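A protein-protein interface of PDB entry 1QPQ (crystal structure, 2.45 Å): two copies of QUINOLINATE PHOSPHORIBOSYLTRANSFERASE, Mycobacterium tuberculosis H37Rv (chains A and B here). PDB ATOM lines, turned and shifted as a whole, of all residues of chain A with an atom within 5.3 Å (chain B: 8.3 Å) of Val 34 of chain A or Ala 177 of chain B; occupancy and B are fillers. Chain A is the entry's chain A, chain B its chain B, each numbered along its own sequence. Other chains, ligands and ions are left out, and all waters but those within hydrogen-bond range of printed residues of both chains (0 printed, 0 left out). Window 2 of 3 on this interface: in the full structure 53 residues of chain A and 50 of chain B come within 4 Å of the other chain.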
ATOM      1  N   THR A  29     -22.915   6.906 -24.297  1.00  0.00           N
ATOM      2  CA  THR A  29     -22.691   6.531 -22.911  1.00  0.00           C
ATOM      3  C   THR A  29     -21.710   5.363 -22.695  1.00  0.00           C
ATOM      4  O   THR A  29     -21.000   5.364 -21.693  1.00  0.00           O
ATOM      5  CB  THR A  29     -24.071   6.374 -22.133  1.00  0.00           C
ATOM      6  OG1 THR A  29     -23.971   5.379 -21.102  1.00  0.00           O
ATOM      7  CG2 THR A  29     -25.216   6.051 -23.075  1.00  0.00           C
ATOM      8  N   THR A  30     -21.653   4.359 -23.581  1.00  0.00           N
ATOM      9  CA  THR A  30     -20.687   3.277 -23.338  1.00  0.00           C
ATOM     10  C   THR A  30     -19.337   3.676 -23.858  1.00  0.00           C
ATOM     11  O   THR A  30     -18.319   3.257 -23.308  1.00  0.00           O
ATOM     12  CB  THR A  30     -21.123   1.858 -23.826  1.00  0.00           C
ATOM     13  OG1 THR A  30     -20.331   1.371 -24.902  1.00  0.00           O
ATOM     14  CG2 THR A  30     -22.478   1.878 -24.228  1.00  0.00           C
ATOM     15  N   LEU A  31     -19.327   4.534 -24.881  1.00  0.00           N
ATOM     16  CA  LEU A  31     -18.071   5.030 -25.441  1.00  0.00           C
ATOM     17  C   LEU A  31     -17.387   5.876 -24.373  1.00  0.00           C
ATOM     18  O   LEU A  31     -16.164   5.806 -24.202  1.00  0.00           O
ATOM     19  CB  LEU A  31     -18.343   5.896 -26.656  1.00  0.00           C
ATOM     20  CG  LEU A  31     -18.212   5.219 -28.015  1.00  0.00           C
ATOM     21  CD1 LEU A  31     -18.814   3.831 -27.982  1.00  0.00           C
ATOM     22  CD2 LEU A  31     -18.885   6.087 -29.062  1.00  0.00           C
ATOM     23  N   ALA A  32     -18.181   6.657 -23.640  1.00  0.00           N
ATOM     24  CA  ALA A  32     -17.630   7.517 -22.605  1.00  0.00           C
ATOM     25  C   ALA A  32     -17.242   6.805 -21.310  1.00  0.00           C
ATOM     26  O   ALA A  32     -16.387   7.296 -20.577  1.00  0.00           O
ATOM     27  CB  ALA A  32     -18.578   8.649 -22.301  1.00  0.00           C
ATOM     28  N   THR A  33     -17.812   5.629 -21.061  1.00  0.00           N
ATOM     29  CA  THR A  33     -17.543   4.900 -19.821  1.00  0.00           C
ATOM     30  C   THR A  33     -16.665   3.641 -19.893  1.00  0.00           C
ATOM     31  O   THR A  33     -15.990   3.282 -18.909  1.00  0.00           O
ATOM     32  CB  THR A  33     -18.900   4.552 -19.083  1.00  0.00           C
ATOM     33  OG1 THR A  33     -19.765   3.768 -19.939  1.00  0.00           O
ATOM     34  CG2 THR A  33     -19.632   5.832 -18.684  1.00  0.00           C
ATOM     35  N   VAL A  34     -16.688   2.941 -21.024  1.00  0.00           N
ATOM     36  CA  VAL A  34     -15.903   1.724 -21.134  1.00  0.00           C
ATOM     37  C   VAL A  34     -14.904   1.791 -22.255  1.00  0.00           C
ATOM     38  O   VAL A  34     -15.192   2.258 -23.341  1.00  0.00           O
ATOM     39  CB  VAL A  34     -16.783   0.435 -21.156  1.00  0.00           C
ATOM     40  CG1 VAL A  34     -18.193   0.763 -21.492  1.00  0.00           C
ATOM     41  CG2 VAL A  34     -16.226  -0.603 -22.081  1.00  0.00           C
ATOM     42  N   PRO A  35     -13.652   1.471 -21.937  1.00  0.00           N
ATOM     43  CA  PRO A  35     -12.599   1.505 -22.928  1.00  0.00           C
ATOM     44  C   PRO A  35     -12.694   0.399 -23.944  1.00  0.00           C
ATOM     45  O   PRO A  35     -13.166  -0.681 -23.671  1.00  0.00           O
ATOM     46  CB  PRO A  35     -11.326   1.438 -22.067  1.00  0.00           C
ATOM     47  CG  PRO A  35     -11.725   0.705 -20.873  1.00  0.00           C
ATOM     48  CD  PRO A  35     -13.082   1.297 -20.584  1.00  0.00           C
ATOM     49  N   ALA A  36     -12.159   0.678 -25.120  1.00  0.00           N
ATOM     50  CA  ALA A  36     -12.151  -0.265 -26.226  1.00  0.00           C
ATOM     51  C   ALA A  36     -11.501  -1.581 -25.844  1.00  0.00           C
ATOM     52  O   ALA A  36     -11.903  -2.647 -26.320  1.00  0.00           O
ATOM     53  CB  ALA A  36     -11.433   0.348 -27.411  1.00  0.00           C
ATOM     54  N   ALA A  38     -11.640  -3.062 -22.994  1.00  0.00           N
ATOM     55  CA  ALA A  38     -12.383  -3.820 -21.977  1.00  0.00           C
ATOM     56  C   ALA A  38     -12.994  -5.119 -22.488  1.00  0.00           C
ATOM     57  O   ALA A  38     -13.479  -5.193 -23.618  1.00  0.00           O
ATOM     58  CB  ALA A  38     -13.438  -2.964 -21.341  1.00  0.00           C
ATOM     59  N   THR A  96     -16.415  -5.621 -23.853  1.00  0.00           N
ATOM     60  CA  THR A  96     -17.494  -4.965 -23.157  1.00  0.00           C
ATOM     61  C   THR A  96     -18.316  -4.013 -23.999  1.00  0.00           C
ATOM     62  O   THR A  96     -19.531  -4.092 -23.995  1.00  0.00           O
ATOM     63  CB  THR A  96     -16.983  -4.272 -21.896  1.00  0.00           C
ATOM     64  OG1 THR A  96     -16.238  -5.225 -21.131  1.00  0.00           O
ATOM     65  CG2 THR A  96     -18.147  -3.784 -21.027  1.00  0.00           C
ATOM     66  N   ARG A  97     -17.678  -3.145 -24.771  1.00  0.00           N
ATOM     67  CA  ARG A  97     -18.433  -2.176 -25.585  1.00  0.00           C
ATOM     68  C   ARG A  97     -19.416  -2.834 -26.538  1.00  0.00           C
ATOM     69  O   ARG A  97     -20.547  -2.360 -26.719  1.00  0.00           O
ATOM     70  CB  ARG A  97     -17.487  -1.307 -26.399  1.00  0.00           C
ATOM     71  CG  ARG A  97     -16.751  -0.247 -25.603  1.00  0.00           C
ATOM     72  CD  ARG A  97     -15.799   0.537 -26.507  1.00  0.00           C
ATOM     73  NE  ARG A  97     -15.384   1.796 -25.899  1.00  0.00           N
ATOM     74  CZ  ARG A  97     -14.667   2.734 -26.507  1.00  0.00           C
ATOM     75  NH1 ARG A  97     -14.264   2.571 -27.759  1.00  0.00           N
ATOM     76  NH2 ARG A  97     -14.376   3.852 -25.862  1.00  0.00           N
ATOM     77  N   LEU A 100     -22.578  -4.125 -24.596  1.00  0.00           N
ATOM     78  CA  LEU A 100     -23.519  -3.095 -24.178  1.00  0.00           C
ATOM     79  C   LEU A 100     -24.318  -2.500 -25.293  1.00  0.00           C
ATOM     80  O   LEU A 100     -25.422  -2.018 -25.099  1.00  0.00           O
ATOM     81  CB  LEU A 100     -22.816  -2.020 -23.350  1.00  0.00           C
ATOM     82  CG  LEU A 100     -22.741  -2.210 -21.814  1.00  0.00           C
ATOM     83  CD1 LEU A 100     -22.662  -3.652 -21.428  1.00  0.00           C
ATOM     84  CD2 LEU A 100     -21.581  -1.446 -21.195  1.00  0.00           C
ATOM     85  N   LYS B 171     -26.682   3.225 -17.242  1.00  0.00           N
ATOM     86  CA  LYS B 171     -27.255   2.023 -16.660  1.00  0.00           C
ATOM     87  C   LYS B 171     -26.271   1.325 -15.753  1.00  0.00           C
ATOM     88  O   LYS B 171     -25.112   1.702 -15.680  1.00  0.00           O
ATOM     89  CB  LYS B 171     -27.685   1.057 -17.762  1.00  0.00           C
ATOM     90  CG  LYS B 171     -28.796   1.609 -18.639  1.00  0.00           C
ATOM     91  CD  LYS B 171     -29.020   0.764 -19.899  1.00  0.00           C
ATOM     92  CE  LYS B 171     -30.377   1.056 -20.487  1.00  0.00           C
ATOM     93  NZ  LYS B 171     -31.465   0.677 -19.527  1.00  0.00           N
ATOM     94  N   ASP B 172     -26.730   0.241 -15.145  1.00  0.00           N
ATOM     95  CA  ASP B 172     -25.935  -0.541 -14.216  1.00  0.00           C
ATOM     96  C   ASP B 172     -24.635  -1.072 -14.778  1.00  0.00           C
ATOM     97  O   ASP B 172     -23.617  -1.135 -14.070  1.00  0.00           O
ATOM     98  CB  ASP B 172     -26.766  -1.690 -13.658  1.00  0.00           C
ATOM     99  CG  ASP B 172     -27.305  -2.603 -14.734  1.00  0.00           C
ATOM    100  OD1 ASP B 172     -27.663  -2.106 -15.829  1.00  0.00           O
ATOM    101  OD2 ASP B 172     -27.386  -3.825 -14.471  1.00  0.00           O
ATOM    102  N   ASN B 173     -24.665  -1.453 -16.051  1.00  0.00           N
ATOM    103  CA  ASN B 173     -23.472  -1.979 -16.698  1.00  0.00           C
ATOM    104  C   ASN B 173     -22.403  -0.900 -16.994  1.00  0.00           C
ATOM    105  O   ASN B 173     -21.218  -1.214 -17.099  1.00  0.00           O
ATOM    106  CB  ASN B 173     -23.871  -2.799 -17.930  1.00  0.00           C
ATOM    107  CG  ASN B 173     -24.567  -4.112 -17.553  1.00  0.00           C
ATOM    108  OD1 ASN B 173     -24.277  -4.709 -16.512  1.00  0.00           O
ATOM    109  ND2 ASN B 173     -25.498  -4.558 -18.389  1.00  0.00           N
ATOM    110  N   HIS B 174     -22.807   0.372 -17.045  1.00  0.00           N
ATOM    111  CA  HIS B 174     -21.863   1.474 -17.290  1.00  0.00           C
ATOM    112  C   HIS B 174     -21.256   1.866 -15.989  1.00  0.00           C
ATOM    113  O   HIS B 174     -20.099   2.219 -15.937  1.00  0.00           O
ATOM    114  CB  HIS B 174     -22.531   2.740 -17.826  1.00  0.00           C
ATOM    115  CG  HIS B 174     -23.246   2.536 -19.117  1.00  0.00           C
ATOM    116  ND1 HIS B 174     -22.637   1.993 -20.226  1.00  0.00           N
ATOM    117  CD2 HIS B 174     -24.538   2.734 -19.457  1.00  0.00           C
ATOM    118  CE1 HIS B 174     -23.527   1.859 -21.192  1.00  0.00           C
ATOM    119  NE2 HIS B 174     -24.687   2.302 -20.750  1.00  0.00           N
ATOM    120  N   VAL B 175     -22.105   1.984 -14.977  1.00  0.00           N
ATOM    121  CA  VAL B 175     -21.668   2.343 -13.636  1.00  0.00           C
ATOM    122  C   VAL B 175     -20.567   1.343 -13.240  1.00  0.00           C
ATOM    123  O   VAL B 175     -19.496   1.746 -12.754  1.00  0.00           O
ATOM    124  CB  VAL B 175     -22.860   2.304 -12.628  1.00  0.00           C
ATOM    125  CG1 VAL B 175     -22.352   2.374 -11.190  1.00  0.00           C
ATOM    126  CG2 VAL B 175     -23.821   3.461 -12.918  1.00  0.00           C
ATOM    127  N   ALA B 176     -20.816   0.057 -13.524  1.00  0.00           N
ATOM    128  CA  ALA B 176     -19.873  -1.032 -13.240  1.00  0.00           C
ATOM    129  C   ALA B 176     -18.570  -0.757 -13.973  1.00  0.00           C
ATOM    130  O   ALA B 176     -17.496  -0.712 -13.367  1.00  0.00           O
ATOM    131  CB  ALA B 176     -20.454  -2.372 -13.708  1.00  0.00           C
ATOM    132  N   ALA B 177     -18.684  -0.551 -15.280  1.00  0.00           N
ATOM    133  CA  ALA B 177     -17.534  -0.265 -16.110  1.00  0.00           C
ATOM    134  C   ALA B 177     -16.814   1.010 -15.658  1.00  0.00           C
ATOM    135  O   ALA B 177     -15.606   1.019 -15.490  1.00  0.00           O
ATOM    136  CB  ALA B 177     -17.972  -0.159 -17.573  1.00  0.00           C
ATOM    137  N   ALA B 178     -17.565   2.068 -15.396  1.00  0.00           N
ATOM    138  CA  ALA B 178     -16.985   3.332 -14.977  1.00  0.00           C
ATOM    139  C   ALA B 178     -16.554   3.267 -13.521  1.00  0.00           C
ATOM    140  O   ALA B 178     -15.915   4.200 -13.014  1.00  0.00           O
ATOM    141  CB  ALA B 178     -17.981   4.447 -15.179  1.00  0.00           C
ATOM    142  N   GLY B 179     -16.949   2.191 -12.844  1.00  0.00           N
ATOM    143  CA  GLY B 179     -16.608   2.005 -11.444  1.00  0.00           C
ATOM    144  C   GLY B 179     -17.447   2.803 -10.451  1.00  0.00           C
ATOM    145  O   GLY B 179     -17.498   2.468  -9.262  1.00  0.00           O
ATOM    146  N   SER B 180     -18.103   3.861 -10.906  1.00  0.00           N
ATOM    147  CA  SER B 180     -18.912   4.653 -10.002  1.00  0.00           C
ATOM    148  C   SER B 180     -19.973   5.419 -10.761  1.00  0.00           C
ATOM    149  O   SER B 180     -19.792   5.745 -11.934  1.00  0.00           O
ATOM    150  CB  SER B 180     -18.027   5.605  -9.191  1.00  0.00           C
ATOM    151  OG  SER B 180     -18.774   6.681  -8.634  1.00  0.00           O
ATOM    152  N   ASP B 183     -18.667   8.834 -11.382  1.00  0.00           N
ATOM    153  CA  ASP B 183     -17.593   8.728 -12.378  1.00  0.00           C
ATOM    154  C   ASP B 183     -18.215   8.690 -13.768  1.00  0.00           C
ATOM    155  O   ASP B 183     -17.945   9.540 -14.616  1.00  0.00           O
ATOM    156  CB  ASP B 183     -16.754   7.464 -12.140  1.00  0.00           C
ATOM    157  CG  ASP B 183     -15.780   7.604 -10.966  1.00  0.00           C
ATOM    158  OD1 ASP B 183     -15.551   8.753 -10.492  1.00  0.00           O
ATOM    159  OD2 ASP B 183     -15.239   6.552 -10.533  1.00  0.00           O
ATOM    160  N   ALA B 184     -19.104   7.722 -13.951  1.00  0.00           N
ATOM    161  CA  ALA B 184     -19.838   7.542 -15.185  1.00  0.00           C
ATOM    162  C   ALA B 184     -20.528   8.842 -15.600  1.00  0.00           C
ATOM    163  O   ALA B 184     -20.361   9.303 -16.736  1.00  0.00           O
ATOM    164  CB  ALA B 184     -20.873   6.438 -14.995  1.00  0.00           C
ATOM    165  N   ALA B 187     -18.079  11.528 -16.655  1.00  0.00           N
ATOM    166  CA  ALA B 187     -17.520  11.084 -17.934  1.00  0.00           C
ATOM    167  C   ALA B 187     -18.406  11.417 -19.126  1.00  0.00           C
ATOM    168  O   ALA B 187     -17.918  11.909 -20.141  1.00  0.00           O
ATOM    169  CB  ALA B 187     -17.254   9.578 -17.901  1.00  0.00           C
ATOM    170  N   VAL B 188     -19.699  11.142 -18.999  1.00  0.00           N
ATOM    171  CA  VAL B 188     -20.657  11.412 -20.054  1.00  0.00           C
ATOM    172  C   VAL B 188     -20.906  12.904 -20.201  1.00  0.00           C
ATOM    173  O   VAL B 188     -21.175  13.381 -21.293  1.00  0.00           O
ATOM    174  CB  VAL B 188     -21.985  10.701 -19.786  1.00  0.00           C
ATOM    175  CG1 VAL B 188     -22.994  11.095 -20.846  1.00  0.00           C
ATOM    176  CG2 VAL B 188     -21.776   9.165 -19.771  1.00  0.00           C
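Thr 30 of chain A touches His 174 of chain B (CG2 to CE1, 3.2 Å).
Ala 32 of chain A touches Ala 187 of chain B.
Ala 184 of chain B touches Thr 33 of chain A (CA to CG2, 3.9 Å).
Ala 177 of chain B touches Val 34 of chain A (CB to CB, 3.8 Å).
Leu 100 of chain A touches Asn 173 of chain B.
CD2 of Leu 100 of chain A touches ND1 of His 174 of chain B (3.7 Å).
Of chain B, only Ala 177 (3.8 Å) comes within 4 Å of Val 34 of chain A.
Of the printed residues of chain A, Ala 177 of chain B touches Val 34 (3.8 Å).
No residue of chain B comes within 4 Å of Pro 35 of chain A.
Printed residues of chain A within 4 Å of His 174 of chain B: Thr 29, Thr 30, Thr 33 and Leu 100.
Printed residues of chain B within 4 Å of Ala 32 of chain A: Ala 187 (3.6 Å).
Of the printed residues of chain A, Ala 187 of chain B touches Ala 32.
Of the printed residues of chain B, Thr 30 of chain A touches His 174.
Printed residues of chain A within 4 Å of Ala 184 of chain B: Thr 33 (3.9 Å).
The nearest residue of chain B that does not touch Val 34 of chain A is His 174 of chain B (4.8 Å).
The nearest printed residue of chain A that does not touch Ala 184 of chain B is Ala 32 of chain A (5.9 Å).
The side-chain hydroxyl (OG1) of Thr 29 of chain A sits close to a ring nitrogen (NE2) of His 174 of chain B (3.2 Å).
OG1 of Thr 33 of chain A is in hydrogen-bond range of ND1 of His 174 of chain B, at 3.4 Å.
Printed residues of chain A that touch a printed residue of chain B: Thr 29, Thr 30, Ala 32, Thr 33, Val 34 and Leu 100.
Along chain A the printed residues that touch a printed residue of chain B span positions 29 to 100.
Among the printed residues, 8 pairs touch across the chains.
No position is printed for both chains.
O of Thr 29 of chain A is in hydrogen-bond range of OG1 of Thr 33 of chain A, 2.7 Å away.
O of Val 34 of chain A lies within hydrogen-bond range of NE of Arg 97 of chain A, 2.6 Å away.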
